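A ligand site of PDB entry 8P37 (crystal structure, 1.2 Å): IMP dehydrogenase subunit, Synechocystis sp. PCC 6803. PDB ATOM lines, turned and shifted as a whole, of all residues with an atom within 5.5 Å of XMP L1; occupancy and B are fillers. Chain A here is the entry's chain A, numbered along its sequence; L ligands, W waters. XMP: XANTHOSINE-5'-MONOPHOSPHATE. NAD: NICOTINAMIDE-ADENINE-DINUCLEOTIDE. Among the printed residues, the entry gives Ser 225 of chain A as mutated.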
ATOM      1  N   SER A  55      16.471 -14.614  23.984  1.00  0.00           N
ATOM      2  CA  SER A  55      17.129 -15.928  23.972  1.00  0.00           C
ATOM      3  C   SER A  55      18.548 -15.838  23.450  1.00  0.00           C
ATOM      4  O   SER A  55      18.860 -15.100  22.507  1.00  0.00           O
ATOM      5  CB  SER A  55      16.361 -16.902  23.080  1.00  0.00           C
ATOM      6  OG  SER A  55      15.026 -17.091  23.529  1.00  0.00           O
ATOM      7  N   ALA A  56      19.389 -16.724  23.964  1.00  0.00           N
ATOM      8  CA  ALA A  56      20.798 -16.879  23.570  1.00  0.00           C
ATOM      9  C   ALA A  56      20.869 -17.703  22.267  1.00  0.00           C
ATOM     10  O   ALA A  56      21.221 -18.900  22.285  1.00  0.00           O
ATOM     11  CB  ALA A  56      21.618 -17.510  24.675  1.00  0.00           C
ATOM     12  N   MET A  57      20.471 -17.064  21.169  1.00  0.00           N
ATOM     13  CA  MET A  57      20.345 -17.648  19.855  1.00  0.00           C
ATOM     14  C   MET A  57      20.912 -16.724  18.844  1.00  0.00           C
ATOM     15  O   MET A  57      20.706 -15.491  18.918  1.00  0.00           O
ATOM     16  CB  MET A  57      18.896 -18.018  19.528  1.00  0.00           C
ATOM     17  CG  MET A  57      18.284 -18.946  20.548  1.00  0.00           C
ATOM     18  SD  MET A  57      16.506 -19.194  20.386  1.00  0.00           S
ATOM     19  CE  MET A  57      16.425 -20.271  18.965  1.00  0.00           C
ATOM     20  N   GLN A 163      22.828 -22.882  30.464  1.00  0.00           N
ATOM     21  CA  GLN A 163      21.595 -23.302  29.822  1.00  0.00           C
ATOM     22  C   GLN A 163      21.832 -24.420  28.862  1.00  0.00           C
ATOM     23  O   GLN A 163      22.691 -24.387  27.990  1.00  0.00           O
ATOM     24  CB  GLN A 163      21.005 -22.086  29.077  1.00  0.00           C
ATOM     25  CG  GLN A 163      19.700 -22.401  28.405  1.00  0.00           C
ATOM     26  CD  GLN A 163      18.984 -21.200  27.859  1.00  0.00           C
ATOM     27  OE1 GLN A 163      19.540 -20.280  27.253  1.00  0.00           O
ATOM     28  NE2 GLN A 163      17.674 -21.238  28.016  1.00  0.00           N
ATOM     29  N   ASN A 197      17.652 -25.695  31.436  1.00  0.00           N
ATOM     30  CA  ASN A 197      16.227 -25.588  31.574  1.00  0.00           C
ATOM     31  C   ASN A 197      15.683 -26.766  32.385  1.00  0.00           C
ATOM     32  O   ASN A 197      16.330 -27.812  32.528  1.00  0.00           O
ATOM     33  CB  ASN A 197      15.579 -25.480  30.182  1.00  0.00           C
ATOM     34  CG  ASN A 197      15.697 -24.131  29.580  1.00  0.00           C
ATOM     35  OD1 ASN A 197      16.738 -23.469  29.759  1.00  0.00           O
ATOM     36  ND2 ASN A 197      14.677 -23.614  28.959  1.00  0.00           N
ATOM     37  N   GLY A 218      11.348 -24.668  30.489  1.00  0.00           N
ATOM     38  CA  GLY A 218      10.854 -25.013  29.161  1.00  0.00           C
ATOM     39  C   GLY A 218      11.724 -26.011  28.450  1.00  0.00           C
ATOM     40  O   GLY A 218      12.945 -25.824  28.326  1.00  0.00           O
ATOM     41  N   GLY A 220      11.528 -27.772  24.770  1.00  0.00           N
ATOM     42  CA  GLY A 220      10.876 -27.915  23.494  1.00  0.00           C
ATOM     43  C   GLY A 220       9.737 -27.036  23.050  1.00  0.00           C
ATOM     44  O   GLY A 220       9.248 -27.325  21.977  1.00  0.00           O
ATOM     45  N   PRO A 221       9.247 -25.990  23.779  1.00  0.00           N
ATOM     46  CA  PRO A 221       8.171 -25.169  23.204  1.00  0.00           C
ATOM     47  C   PRO A 221       8.615 -24.264  22.057  1.00  0.00           C
ATOM     48  O   PRO A 221       7.763 -23.661  21.431  1.00  0.00           O
ATOM     49  CB  PRO A 221       7.700 -24.368  24.404  1.00  0.00           C
ATOM     50  CG  PRO A 221       8.973 -24.127  25.217  1.00  0.00           C
ATOM     51  CD  PRO A 221       9.696 -25.470  25.084  1.00  0.00           C
ATOM     52  N   GLY A 222       9.928 -24.112  21.828  1.00  0.00           N
ATOM     53  CA  GLY A 222      10.427 -23.106  20.888  1.00  0.00           C
ATOM     54  C   GLY A 222       9.920 -23.183  19.487  1.00  0.00           C
ATOM     55  O   GLY A 222       9.737 -24.268  18.922  1.00  0.00           O
ATOM     56  N   ALA A 223       9.809 -22.014  18.866  1.00  0.00           N
ATOM     57  CA  ALA A 223       9.416 -21.946  17.465  1.00  0.00           C
ATOM     58  C   ALA A 223      10.421 -22.621  16.522  1.00  0.00           C
ATOM     59  O   ALA A 223      10.040 -23.069  15.430  1.00  0.00           O
ATOM     60  CB  ALA A 223       9.220 -20.500  17.058  1.00  0.00           C
ATOM     61  N   ALA A 224      11.701 -22.667  16.904  1.00  0.00           N
ATOM     62  CA  ALA A 224      12.740 -23.292  16.094  1.00  0.00           C
ATOM     63  C   ALA A 224      13.247 -24.591  16.748  1.00  0.00           C
ATOM     64  O   ALA A 224      14.329 -25.090  16.431  1.00  0.00           O
ATOM     65  CB  ALA A 224      13.885 -22.305  15.871  1.00  0.00           C
ATOM     66  N   SER A 225      12.440 -25.166  17.684  1.00  0.00           N
ATOM     67  CA  SER A 225      12.783 -26.347  18.418  1.00  0.00           C
ATOM     68  C   SER A 225      12.240 -27.586  17.763  1.00  0.00           C
ATOM     69  O   SER A 225      11.085 -27.622  17.368  1.00  0.00           O
ATOM     70  CB  SER A 225      12.147 -26.253  19.788  1.00  0.00           C
ATOM     71  OG  SER A 225      12.196 -27.496  20.477  1.00  0.00           O
ATOM     72  N   THR A 226      13.069 -28.634  17.706  1.00  0.00           N
ATOM     73  CA  THR A 226      12.572 -29.960  17.285  1.00  0.00           C
ATOM     74  C   THR A 226      12.810 -31.023  18.350  1.00  0.00           C
ATOM     75  O   THR A 226      12.498 -32.184  18.095  1.00  0.00           O
ATOM     76  CB  THR A 226      13.095 -30.401  15.962  1.00  0.00           C
ATOM     77  OG1 THR A 226      14.500 -30.642  16.058  1.00  0.00           O
ATOM     78  CG2 THR A 226      12.838 -29.404  14.893  1.00  0.00           C
ATOM     79  N   SER A 227      13.237 -30.648  19.572  1.00  0.00           N
ATOM     80  CA  SER A 227      13.496 -31.630  20.625  1.00  0.00           C
ATOM     81  C   SER A 227      12.340 -32.516  20.995  1.00  0.00           C
ATOM     82  O   SER A 227      12.540 -33.696  21.312  1.00  0.00           O
ATOM     83  CB  SER A 227      14.007 -30.981  21.900  1.00  0.00           C
ATOM     84  OG  SER A 227      15.262 -30.340  21.687  1.00  0.00           O
ATOM     85  N   ARG A 228      11.108 -32.005  20.974  1.00  0.00           N
ATOM     86  CA  ARG A 228       9.974 -32.810  21.331  1.00  0.00           C
ATOM     87  C   ARG A 228       9.739 -33.926  20.310  1.00  0.00           C
ATOM     88  O   ARG A 228       9.397 -35.037  20.655  1.00  0.00           O
ATOM     89  CB  ARG A 228       8.735 -31.967  21.550  1.00  0.00           C
ATOM     90  CG  ARG A 228       8.770 -31.140  22.817  1.00  0.00           C
ATOM     91  CD  ARG A 228       7.737 -30.058  22.830  1.00  0.00           C
ATOM     92  NE  ARG A 228       7.751 -29.328  24.083  1.00  0.00           N
ATOM     93  CZ  ARG A 228       6.821 -28.475  24.496  1.00  0.00           C
ATOM     94  NH1 ARG A 228       5.710 -28.296  23.779  1.00  0.00           N
ATOM     95  NH2 ARG A 228       6.947 -27.854  25.659  1.00  0.00           N
ATOM     96  N   ASP A 264      10.561 -19.863  29.270  1.00  0.00           N
ATOM     97  CA  ASP A 264      11.424 -19.762  28.117  1.00  0.00           C
ATOM     98  C   ASP A 264      10.912 -20.447  26.864  1.00  0.00           C
ATOM     99  O   ASP A 264      10.864 -21.679  26.786  1.00  0.00           O
ATOM    100  CB  ASP A 264      12.781 -20.382  28.505  1.00  0.00           C
ATOM    101  CG  ASP A 264      13.812 -20.379  27.410  1.00  0.00           C
ATOM    102  OD1 ASP A 264      13.606 -19.696  26.420  1.00  0.00           O
ATOM    103  OD2 ASP A 264      14.863 -21.073  27.564  1.00  0.00           O
ATOM    104  N   GLY A 265      10.480 -19.643  25.883  1.00  0.00           N
ATOM    105  CA  GLY A 265      10.163 -20.120  24.540  1.00  0.00           C
ATOM    106  C   GLY A 265       8.712 -20.414  24.246  1.00  0.00           C
ATOM    107  O   GLY A 265       7.875 -20.512  25.148  1.00  0.00           O
ATOM    108  N   GLY A 266       8.446 -20.513  22.968  1.00  0.00           N
ATOM    109  CA  GLY A 266       7.103 -20.801  22.499  1.00  0.00           C
ATOM    110  C   GLY A 266       6.157 -19.638  22.528  1.00  0.00           C
ATOM    111  O   GLY A 266       4.957 -19.802  22.309  1.00  0.00           O
ATOM    112  N   ILE A 267       6.677 -18.449  22.751  1.00  0.00           N
ATOM    113  CA  ILE A 267       5.881 -17.208  22.833  1.00  0.00           C
ATOM    114  C   ILE A 267       6.009 -16.489  21.511  1.00  0.00           C
ATOM    115  O   ILE A 267       7.127 -16.204  21.055  1.00  0.00           O
ATOM    116  CB  ILE A 267       6.415 -16.344  23.985  1.00  0.00           C
ATOM    117  CG1 ILE A 267       6.028 -16.990  25.346  1.00  0.00           C
ATOM    118  CG2 ILE A 267       5.985 -14.864  23.893  1.00  0.00           C
ATOM    119  CD1 ILE A 267       6.880 -16.532  26.491  1.00  0.00           C
ATOM    120  N   MET A 285      11.590 -15.490  28.533  1.00  0.00           N
ATOM    121  CA  MET A 285      12.690 -15.509  27.601  1.00  0.00           C
ATOM    122  C   MET A 285      12.107 -15.863  26.257  1.00  0.00           C
ATOM    123  O   MET A 285      11.393 -16.875  26.112  1.00  0.00           O
ATOM    124  CB  MET A 285      13.786 -16.453  28.047  1.00  0.00           C
ATOM    125  CG  MET A 285      14.883 -16.616  27.005  1.00  0.00           C
ATOM    126  SD  MET A 285      16.191 -17.712  27.471  1.00  0.00           S
ATOM    127  CE  MET A 285      17.304 -16.593  28.208  1.00  0.00           C
ATOM    128  N   ILE A 286      12.340 -14.981  25.251  1.00  0.00           N
ATOM    129  CA  ILE A 286      11.757 -15.128  23.928  1.00  0.00           C
ATOM    130  C   ILE A 286      12.814 -14.916  22.871  1.00  0.00           C
ATOM    131  O   ILE A 286      13.756 -14.108  23.047  1.00  0.00           O
ATOM    132  CB  ILE A 286      10.556 -14.164  23.730  1.00  0.00           C
ATOM    133  CG1 ILE A 286      10.996 -12.723  23.566  1.00  0.00           C
ATOM    134  CG2 ILE A 286       9.554 -14.361  24.870  1.00  0.00           C
ATOM    135  CD1 ILE A 286       9.858 -11.722  23.451  1.00  0.00           C
ATOM    136  N   GLY A 287      12.699 -15.631  21.758  1.00  0.00           N
ATOM    137  CA  GLY A 287      13.620 -15.514  20.647  1.00  0.00           C
ATOM    138  C   GLY A 287      12.943 -15.079  19.402  1.00  0.00           C
ATOM    139  O   GLY A 287      13.310 -14.043  18.824  1.00  0.00           O
ATOM    140  N   SER A 288      11.981 -15.909  18.901  1.00  0.00           N
ATOM    141  CA  SER A 288      11.396 -15.608  17.606  1.00  0.00           C
ATOM    142  C   SER A 288      10.786 -14.193  17.511  1.00  0.00           C
ATOM    143  O   SER A 288      10.951 -13.586  16.434  1.00  0.00           O
ATOM    144  CB  SER A 288      10.377 -16.672  17.180  1.00  0.00           C
ATOM    145  OG  SER A 288       9.086 -16.451  17.735  1.00  0.00           O
ATOM    146  N   PRO A 289      10.134 -13.658  18.526  1.00  0.00           N
ATOM    147  CA  PRO A 289       9.570 -12.309  18.357  1.00  0.00           C
ATOM    148  C   PRO A 289      10.618 -11.223  18.150  1.00  0.00           C
ATOM    149  O   PRO A 289      10.327 -10.166  17.587  1.00  0.00           O
ATOM    150  CB  PRO A 289       8.788 -12.083  19.643  1.00  0.00           C
ATOM    151  CG  PRO A 289       8.481 -13.435  20.107  1.00  0.00           C
ATOM    152  CD  PRO A 289       9.710 -14.224  19.826  1.00  0.00           C
ATOM    153  N   HIS A 302      15.534 -17.490  11.862  1.00  0.00           N
ATOM    154  CA  HIS A 302      15.644 -17.843  13.272  1.00  0.00           C
ATOM    155  C   HIS A 302      15.874 -19.331  13.363  1.00  0.00           C
ATOM    156  O   HIS A 302      15.106 -20.106  12.791  1.00  0.00           O
ATOM    157  CB  HIS A 302      14.351 -17.405  13.979  1.00  0.00           C
ATOM    158  CG  HIS A 302      14.295 -17.787  15.423  1.00  0.00           C
ATOM    159  ND1 HIS A 302      15.263 -17.369  16.328  1.00  0.00           N
ATOM    160  CD2 HIS A 302      13.320 -18.412  16.083  1.00  0.00           C
ATOM    161  CE1 HIS A 302      14.826 -17.773  17.512  1.00  0.00           C
ATOM    162  NE2 HIS A 302      13.662 -18.422  17.413  1.00  0.00           N
ATOM    163  N   TRP A 303      16.952 -19.760  13.984  1.00  0.00           N
ATOM    164  CA  TRP A 303      17.296 -21.179  14.083  1.00  0.00           C
ATOM    165  C   TRP A 303      17.624 -21.625  15.491  1.00  0.00           C
ATOM    166  O   TRP A 303      18.120 -20.824  16.333  1.00  0.00           O
ATOM    167  CB  TRP A 303      18.459 -21.539  13.138  1.00  0.00           C
ATOM    168  CG  TRP A 303      19.705 -20.757  13.344  1.00  0.00           C
ATOM    169  CD1 TRP A 303      20.779 -21.114  14.104  1.00  0.00           C
ATOM    170  CD2 TRP A 303      20.017 -19.468  12.797  1.00  0.00           C
ATOM    171  NE1 TRP A 303      21.765 -20.165  14.000  1.00  0.00           N
ATOM    172  CE2 TRP A 303      21.321 -19.142  13.202  1.00  0.00           C
ATOM    173  CE3 TRP A 303      19.336 -18.578  11.949  1.00  0.00           C
ATOM    174  CZ2 TRP A 303      21.959 -17.964  12.795  1.00  0.00           C
ATOM    175  CZ3 TRP A 303      19.928 -17.385  11.610  1.00  0.00           C
ATOM    176  CH2 TRP A 303      21.227 -17.077  12.040  1.00  0.00           C
ATOM    177  N   GLY A 304      17.355 -22.900  15.762  1.00  0.00           N
ATOM    178  CA  GLY A 304      17.678 -23.456  17.049  1.00  0.00           C
ATOM    179  C   GLY A 304      19.174 -23.638  17.165  1.00  0.00           C
ATOM    180  O   GLY A 304      19.859 -23.940  16.187  1.00  0.00           O
ATOM    181  N   MET A 305      19.697 -23.490  18.376  1.00  0.00           N
ATOM    182  CA  MET A 305      21.138 -23.648  18.648  1.00  0.00           C
ATOM    183  C   MET A 305      21.585 -25.089  18.767  1.00  0.00           C
ATOM    184  O   MET A 305      22.779 -25.294  18.840  1.00  0.00           O
ATOM    185  CB  MET A 305      21.534 -22.830  19.889  1.00  0.00           C
ATOM    186  CG  MET A 305      21.391 -21.301  19.673  1.00  0.00           C
ATOM    187  SD  MET A 305      22.398 -20.654  18.337  1.00  0.00           S
ATOM    188  CE  MET A 305      23.948 -20.673  19.156  1.00  0.00           C
ATOM    189  N   ALA A 306      20.677 -26.071  18.645  1.00  0.00           N
ATOM    190  CA  ALA A 306      21.038 -27.464  18.476  1.00  0.00           C
ATOM    191  C   ALA A 306      20.838 -27.942  17.034  1.00  0.00           C
ATOM    192  O   ALA A 306      21.125 -29.100  16.734  1.00  0.00           O
ATOM    193  CB  ALA A 306      20.297 -28.335  19.436  1.00  0.00           C
ATOM    194  N   THR A 307      20.421 -27.071  16.100  1.00  0.00           N
ATOM    195  CA  THR A 307      20.379 -27.385  14.675  1.00  0.00           C
ATOM    196  C   THR A 307      21.790 -27.792  14.182  1.00  0.00           C
ATOM    197  O   THR A 307      21.875 -28.736  13.397  1.00  0.00           O
ATOM    198  CB  THR A 307      19.899 -26.207  13.807  1.00  0.00           C
ATOM    199  OG1 THR A 307      18.738 -25.610  14.382  1.00  0.00           O
ATOM    200  CG2 THR A 307      19.562 -26.647  12.373  1.00  0.00           C
ATOM    201  N   ARG A 314      18.597 -30.965  16.836  1.00  0.00           N
ATOM    202  CA  ARG A 314      17.373 -30.838  17.628  1.00  0.00           C
ATOM    203  C   ARG A 314      16.761 -29.437  17.549  1.00  0.00           C
ATOM    204  O   ARG A 314      15.964 -29.022  18.381  1.00  0.00           O
ATOM    205  CB  ARG A 314      17.671 -31.225  19.068  1.00  0.00           C
ATOM    206  CG  ARG A 314      17.837 -32.738  19.242  1.00  0.00           C
ATOM    207  CD  ARG A 314      18.601 -33.119  20.484  1.00  0.00           C
ATOM    208  NE  ARG A 314      20.012 -32.744  20.263  1.00  0.00           N
ATOM    209  CZ  ARG A 314      20.662 -31.726  20.803  1.00  0.00           C
ATOM    210  NH1 ARG A 314      20.116 -31.020  21.792  1.00  0.00           N
ATOM    211  NH2 ARG A 314      21.923 -31.473  20.451  1.00  0.00           N
ATOM    212  N   GLY A 315      17.051 -28.733  16.461  1.00  0.00           N
ATOM    213  CA  GLY A 315      16.444 -27.452  16.130  1.00  0.00           C
ATOM    214  C   GLY A 315      16.347 -27.370  14.629  1.00  0.00           C
ATOM    215  O   GLY A 315      16.903 -28.201  13.908  1.00  0.00           O
ATOM    216  N   THR A 316      15.604 -26.383  14.151  1.00  0.00           N
ATOM    217  CA  THR A 316      15.495 -26.109  12.716  1.00  0.00           C
ATOM    218  C   THR A 316      15.679 -24.626  12.464  1.00  0.00           C
ATOM    219  O   THR A 316      15.844 -23.830  13.378  1.00  0.00           O
ATOM    220  CB  THR A 316      14.121 -26.627  12.201  1.00  0.00           C
ATOM    221  OG1 THR A 316      14.141 -26.569  10.745  1.00  0.00           O
ATOM    222  CG2 THR A 316      12.979 -25.873  12.764  1.00  0.00           C
HETATM  223  P   XMP L   1      11.372 -19.306  20.557  1.00  0.00           P
HETATM  224  O1P XMP L   1      11.405 -17.842  20.885  1.00  0.00           O
HETATM  225  O2P XMP L   1      12.175 -19.696  19.356  1.00  0.00           O
HETATM  226  O5' XMP L   1      12.055 -20.100  21.845  1.00  0.00           O
HETATM  227  O3P XMP L   1       9.952 -19.884  20.551  1.00  0.00           O
HETATM  228  C5' XMP L   1      13.367 -19.823  22.151  1.00  0.00           C
HETATM  229  C4' XMP L   1      13.913 -20.868  23.109  1.00  0.00           C
HETATM  230  O4' XMP L   1      14.085 -22.100  22.378  1.00  0.00           O
HETATM  231  C1' XMP L   1      15.059 -22.876  23.015  1.00  0.00           C
HETATM  232  N9  XMP L   1      15.997 -23.379  21.989  1.00  0.00           N
HETATM  233  C4  XMP L   1      15.906 -24.597  21.407  1.00  0.00           C
HETATM  234  N3  XMP L   1      15.078 -25.649  21.706  1.00  0.00           N
HETATM  235  N1  XMP L   1      16.239 -26.847  20.061  1.00  0.00           N
HETATM  236  C2  XMP L   1      15.287 -26.817  21.058  1.00  0.00           C
HETATM  237  O2  XMP L   1      14.560 -27.793  21.233  1.00  0.00           O
HETATM  238  C6  XMP L   1      17.075 -25.841  19.697  1.00  0.00           C
HETATM  239  O6  XMP L   1      17.878 -26.037  18.793  1.00  0.00           O
HETATM  240  C5  XMP L   1      16.930 -24.702  20.493  1.00  0.00           C
HETATM  241  N7  XMP L   1      17.559 -23.462  20.480  1.00  0.00           N
HETATM  242  C8  XMP L   1      16.974 -22.709  21.365  1.00  0.00           C
HETATM  243  C2' XMP L   1      15.754 -22.008  24.094  1.00  0.00           C
HETATM  244  O2' XMP L   1      15.168 -22.425  25.353  1.00  0.00           O
HETATM  245  C3' XMP L   1      15.324 -20.603  23.611  1.00  0.00           C
HETATM  246  O3' XMP L   1      15.372 -19.627  24.625  1.00  0.00           O
HETATM  247  PA  NAD L   2      24.212 -29.895  24.742  1.00  0.00           P
HETATM  248  O1A NAD L   2      23.632 -31.015  24.038  1.00  0.00           O
HETATM  249  O2A NAD L   2      25.573 -29.485  24.324  1.00  0.00           O
HETATM  250  O5B NAD L   2      24.324 -30.042  26.399  1.00  0.00           O
HETATM  251  C5B NAD L   2      23.304 -30.566  27.208  1.00  0.00           C
HETATM  252  C4B NAD L   2      23.702 -31.747  27.870  1.00  0.00           C
HETATM  253  O4B NAD L   2      24.521 -31.373  29.066  1.00  0.00           O
HETATM  254  C3B NAD L   2      22.497 -32.426  28.646  1.00  0.00           C
HETATM  255  O3B NAD L   2      21.700 -33.199  27.635  1.00  0.00           O
HETATM  256  C2B NAD L   2      23.068 -33.199  29.511  1.00  0.00           C
HETATM  257  O2B NAD L   2      23.572 -34.513  28.984  1.00  0.00           O
HETATM  258  C1B NAD L   2      24.400 -32.325  29.995  1.00  0.00           C
HETATM  259  N9A NAD L   2      24.285 -31.806  31.332  1.00  0.00           N
HETATM  260  C8A NAD L   2      23.323 -31.535  32.195  1.00  0.00           C
HETATM  261  N7A NAD L   2      23.856 -31.147  33.342  1.00  0.00           N
HETATM  262  C5A NAD L   2      25.180 -31.278  33.201  1.00  0.00           C
HETATM  263  C6A NAD L   2      26.155 -31.118  34.126  1.00  0.00           C
HETATM  264  N6A NAD L   2      26.055 -30.579  35.441  1.00  0.00           N
HETATM  265  N1A NAD L   2      27.413 -31.306  33.756  1.00  0.00           N
HETATM  266  C2A NAD L   2      27.708 -31.712  32.491  1.00  0.00           C
HETATM  267  N3A NAD L   2      26.724 -31.935  31.598  1.00  0.00           N
HETATM  268  C4A NAD L   2      25.470 -31.726  31.975  1.00  0.00           C
HETATM  269  O3  NAD L   2      23.273 -28.623  24.590  1.00  0.00           O
HETATM  270  PN  NAD L   2      21.741 -28.461  24.166  1.00  0.00           P
HETATM  271  O1N NAD L   2      20.844 -29.034  25.218  1.00  0.00           O
HETATM  272  O2N NAD L   2      21.574 -28.886  22.760  1.00  0.00           O
HETATM  273  O5D NAD L   2      21.601 -26.821  24.243  1.00  0.00           O
HETATM  274  C5D NAD L   2      22.435 -26.056  23.383  1.00  0.00           C
HETATM  275  C4D NAD L   2      21.812 -24.812  23.058  1.00  0.00           C
HETATM  276  O4D NAD L   2      20.490 -24.948  22.373  1.00  0.00           O
HETATM  277  C3D NAD L   2      21.432 -23.882  24.300  1.00  0.00           C
HETATM  278  O3D NAD L   2      21.586 -22.452  23.841  1.00  0.00           O
HETATM  279  C2D NAD L   2      20.158 -24.199  24.597  1.00  0.00           C
HETATM  280  O2D NAD L   2      19.306 -23.122  25.175  1.00  0.00           O
HETATM  281  C1D NAD L   2      19.467 -24.670  23.189  1.00  0.00           C
HETATM  282  N1N NAD L   2      18.589 -25.810  23.360  1.00  0.00           N
HETATM  283  C2N NAD L   2      17.486 -25.684  24.108  1.00  0.00           C
HETATM  284  C3N NAD L   2      16.569 -26.725  24.181  1.00  0.00           C
HETATM  285  C7N NAD L   2      15.312 -26.618  25.023  1.00  0.00           C
HETATM  286  O7N NAD L   2      14.338 -27.301  24.780  1.00  0.00           O
HETATM  287  N7N NAD L   2      15.223 -25.629  26.058  1.00  0.00           N
HETATM  288  C4N NAD L   2      16.746 -27.848  23.441  1.00  0.00           C
HETATM  289  C5N NAD L   2      17.838 -27.944  22.645  1.00  0.00           C
HETATM  290  C6N NAD L   2      18.724 -26.920  22.613  1.00  0.00           C
HETATM  291  O   HOH W   1       9.362 -17.143  22.497  1.00  0.00           O
HETATM  292  O   HOH W   2      12.354 -25.115  23.074  1.00  0.00           O
HETATM  293  O   HOH W   3      18.197 -19.189  25.136  1.00  0.00           O
HETATM  294  O   HOH W   4       8.170 -18.275  19.392  1.00  0.00           O
HETATM  295  O   HOH W   5      19.092 -20.988  23.289  1.00  0.00           O
HETATM  296  O   HOH W   6      12.572 -23.534  25.453  1.00  0.00           O
HETATM  297  O   HOH W   7      13.353 -22.084  19.338  1.00  0.00           O
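N of Ser 227 lies within hydrogen-bond range of OG of Ser 225.
The backbone carbonyl oxygen (O) of Gly 218 is in hydrogen-bond range of the side-chain amide nitrogen (ND2) of Asn 197, at 2.9 Å.
The side-chain carboxylate of Asp 264 sits at hydrogen-bond distance from the side-chain amide nitrogen of Gln 163 (2.9 Å).
The backbone NH of Gly 265 lies within hydrogen-bond range of the backbone carbonyl oxygen of Met 285, 2.9 Å away.
The backbone NH of Arg 314 sits at hydrogen-bond distance from the backbone carbonyl oxygen of Ala 306 (3.1 Å).
The backbone NH of Thr 226 is in hydrogen-bond range of the backbone carbonyl oxygen of Arg 314 (3.0 Å).
The backbone NH (N) of Gly 287 sits at hydrogen-bond distance from the side-chain hydroxyl (OG) of Ser 55, 3.3 Å away.
The backbone NH (N) of Ser 227 sits at hydrogen-bond distance from the backbone carbonyl oxygen (O) of Arg 314 (3.4 Å).
The backbone carbonyl oxygen (O) of Gly 218 lies within hydrogen-bond range of a nitrogen (N7N) of NAD L2 (3.2 Å).
The backbone NH (N) of Gly 220 lies within hydrogen-bond range of an oxygen (O7N) of NAD L2 (2.8 Å).
The backbone NH of Ala 306 is in hydrogen-bond range of an oxygen (O6) of XMP L1, 2.8 Å away.
The backbone NH (N) of Ser 288 lies within hydrogen-bond range of an oxygen (O1P) of XMP L1 (2.8 Å).
An oxygen (O2) of XMP L1 lies within hydrogen-bond range of the side-chain hydroxyl (OG) of Ser 225 (2.5 Å).
N of Ala 223 lies within hydrogen-bond range of O3P of XMP L1, at 2.7 Å.
O2 of XMP L1 sits at hydrogen-bond distance from OG of Ser 227 (2.7 Å).
A ring nitrogen (NE2) of His 302 is in hydrogen-bond range of an oxygen (O2P) of XMP L1, at 2.8 Å.
The backbone NH (N) of Met 305 sits at hydrogen-bond distance from a nitrogen (N7) of XMP L1 (3.0 Å).
An oxygen (O1P) of XMP L1 sits at hydrogen-bond distance from the backbone NH (N) of Gly 287, at 2.7 Å.
The side-chain sulfur of Met 285 sits at hydrogen-bond distance from an oxygen (O3') of XMP L1.
OG of Ser 55 sits at hydrogen-bond distance from O3' of XMP L1, at 2.8 Å.
An oxygen (O3P) of XMP L1 sits at hydrogen-bond distance from the backbone NH (N) of Gly 266 (2.9 Å).
The side-chain carboxylate of Asp 264 is in hydrogen-bond range of an oxygen (O3') of XMP L1, 2.5 Å away.
O of Arg 314 is in hydrogen-bond range of N1 of XMP L1 (2.8 Å).
O2N of NAD L2 is in salt-bridge range of NH1 of Arg 314 (2.8 Å).
Met 57 touches XMP L1 (CE to C8, 3.5 Å).
NE2 of Gln 163 touches O2' of XMP L1 (3.8 Å).
Asn 197 touches XMP L1.
Gly 222 touches XMP L1.
Ala 224 touches XMP L1.
Thr 226 touches XMP L1 (N to O2, 3.9 Å).
CA of Gly 265 touches O5' of XMP L1, 3.3 Å away.
C of Ile 286 touches O1P of XMP L1 (3.8 Å).
Gly 304 touches XMP L1.
N of Thr 307 touches O6 of XMP L1, 3.8 Å away.
Gly 315 touches XMP L1.
Of the 33 residues printed, 24 come within 4 Å of XMP L1.
The nearest printed residue that does not touch XMP L1 is Pro 289 (4.1 Å).
A nitrogen (N7N) of NAD L2 sits at hydrogen-bond distance from an oxygen (O2') of XMP L1, 3.3 Å away.
Water W7 bridges an oxygen (O2P) of XMP L1 (2.7 Å) and the backbone NH of Ala 224 (3.0 Å).
Water W4 lies within hydrogen-bond range of OG of Ser 288, O3P of XMP L1 and O of Ile 267.
Water W1 bridges O1P of XMP L1 (2.7 Å) and O of Ile 267 (2.8 Å).
Water W6 lies within hydrogen-bond range of an oxygen (O2') of XMP L1 (2.8 Å), the backbone carbonyl oxygen (O) of Asp 264 (2.9 Å) and a nitrogen (N7N) of NAD L2 (3.4 Å).
Water W3 lies within hydrogen-bond range of the side-chain amide oxygen (OE1) of Gln 163 (2.7 Å), an oxygen (O3') of XMP L1 (2.9 Å), the backbone NH (N) of Ala 56 (3.0 Å) and the side-chain sulfur (SD) of Met 285 (3.4 Å).
Water W5 bridges O2D of NAD L2 and O of Ala 56.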
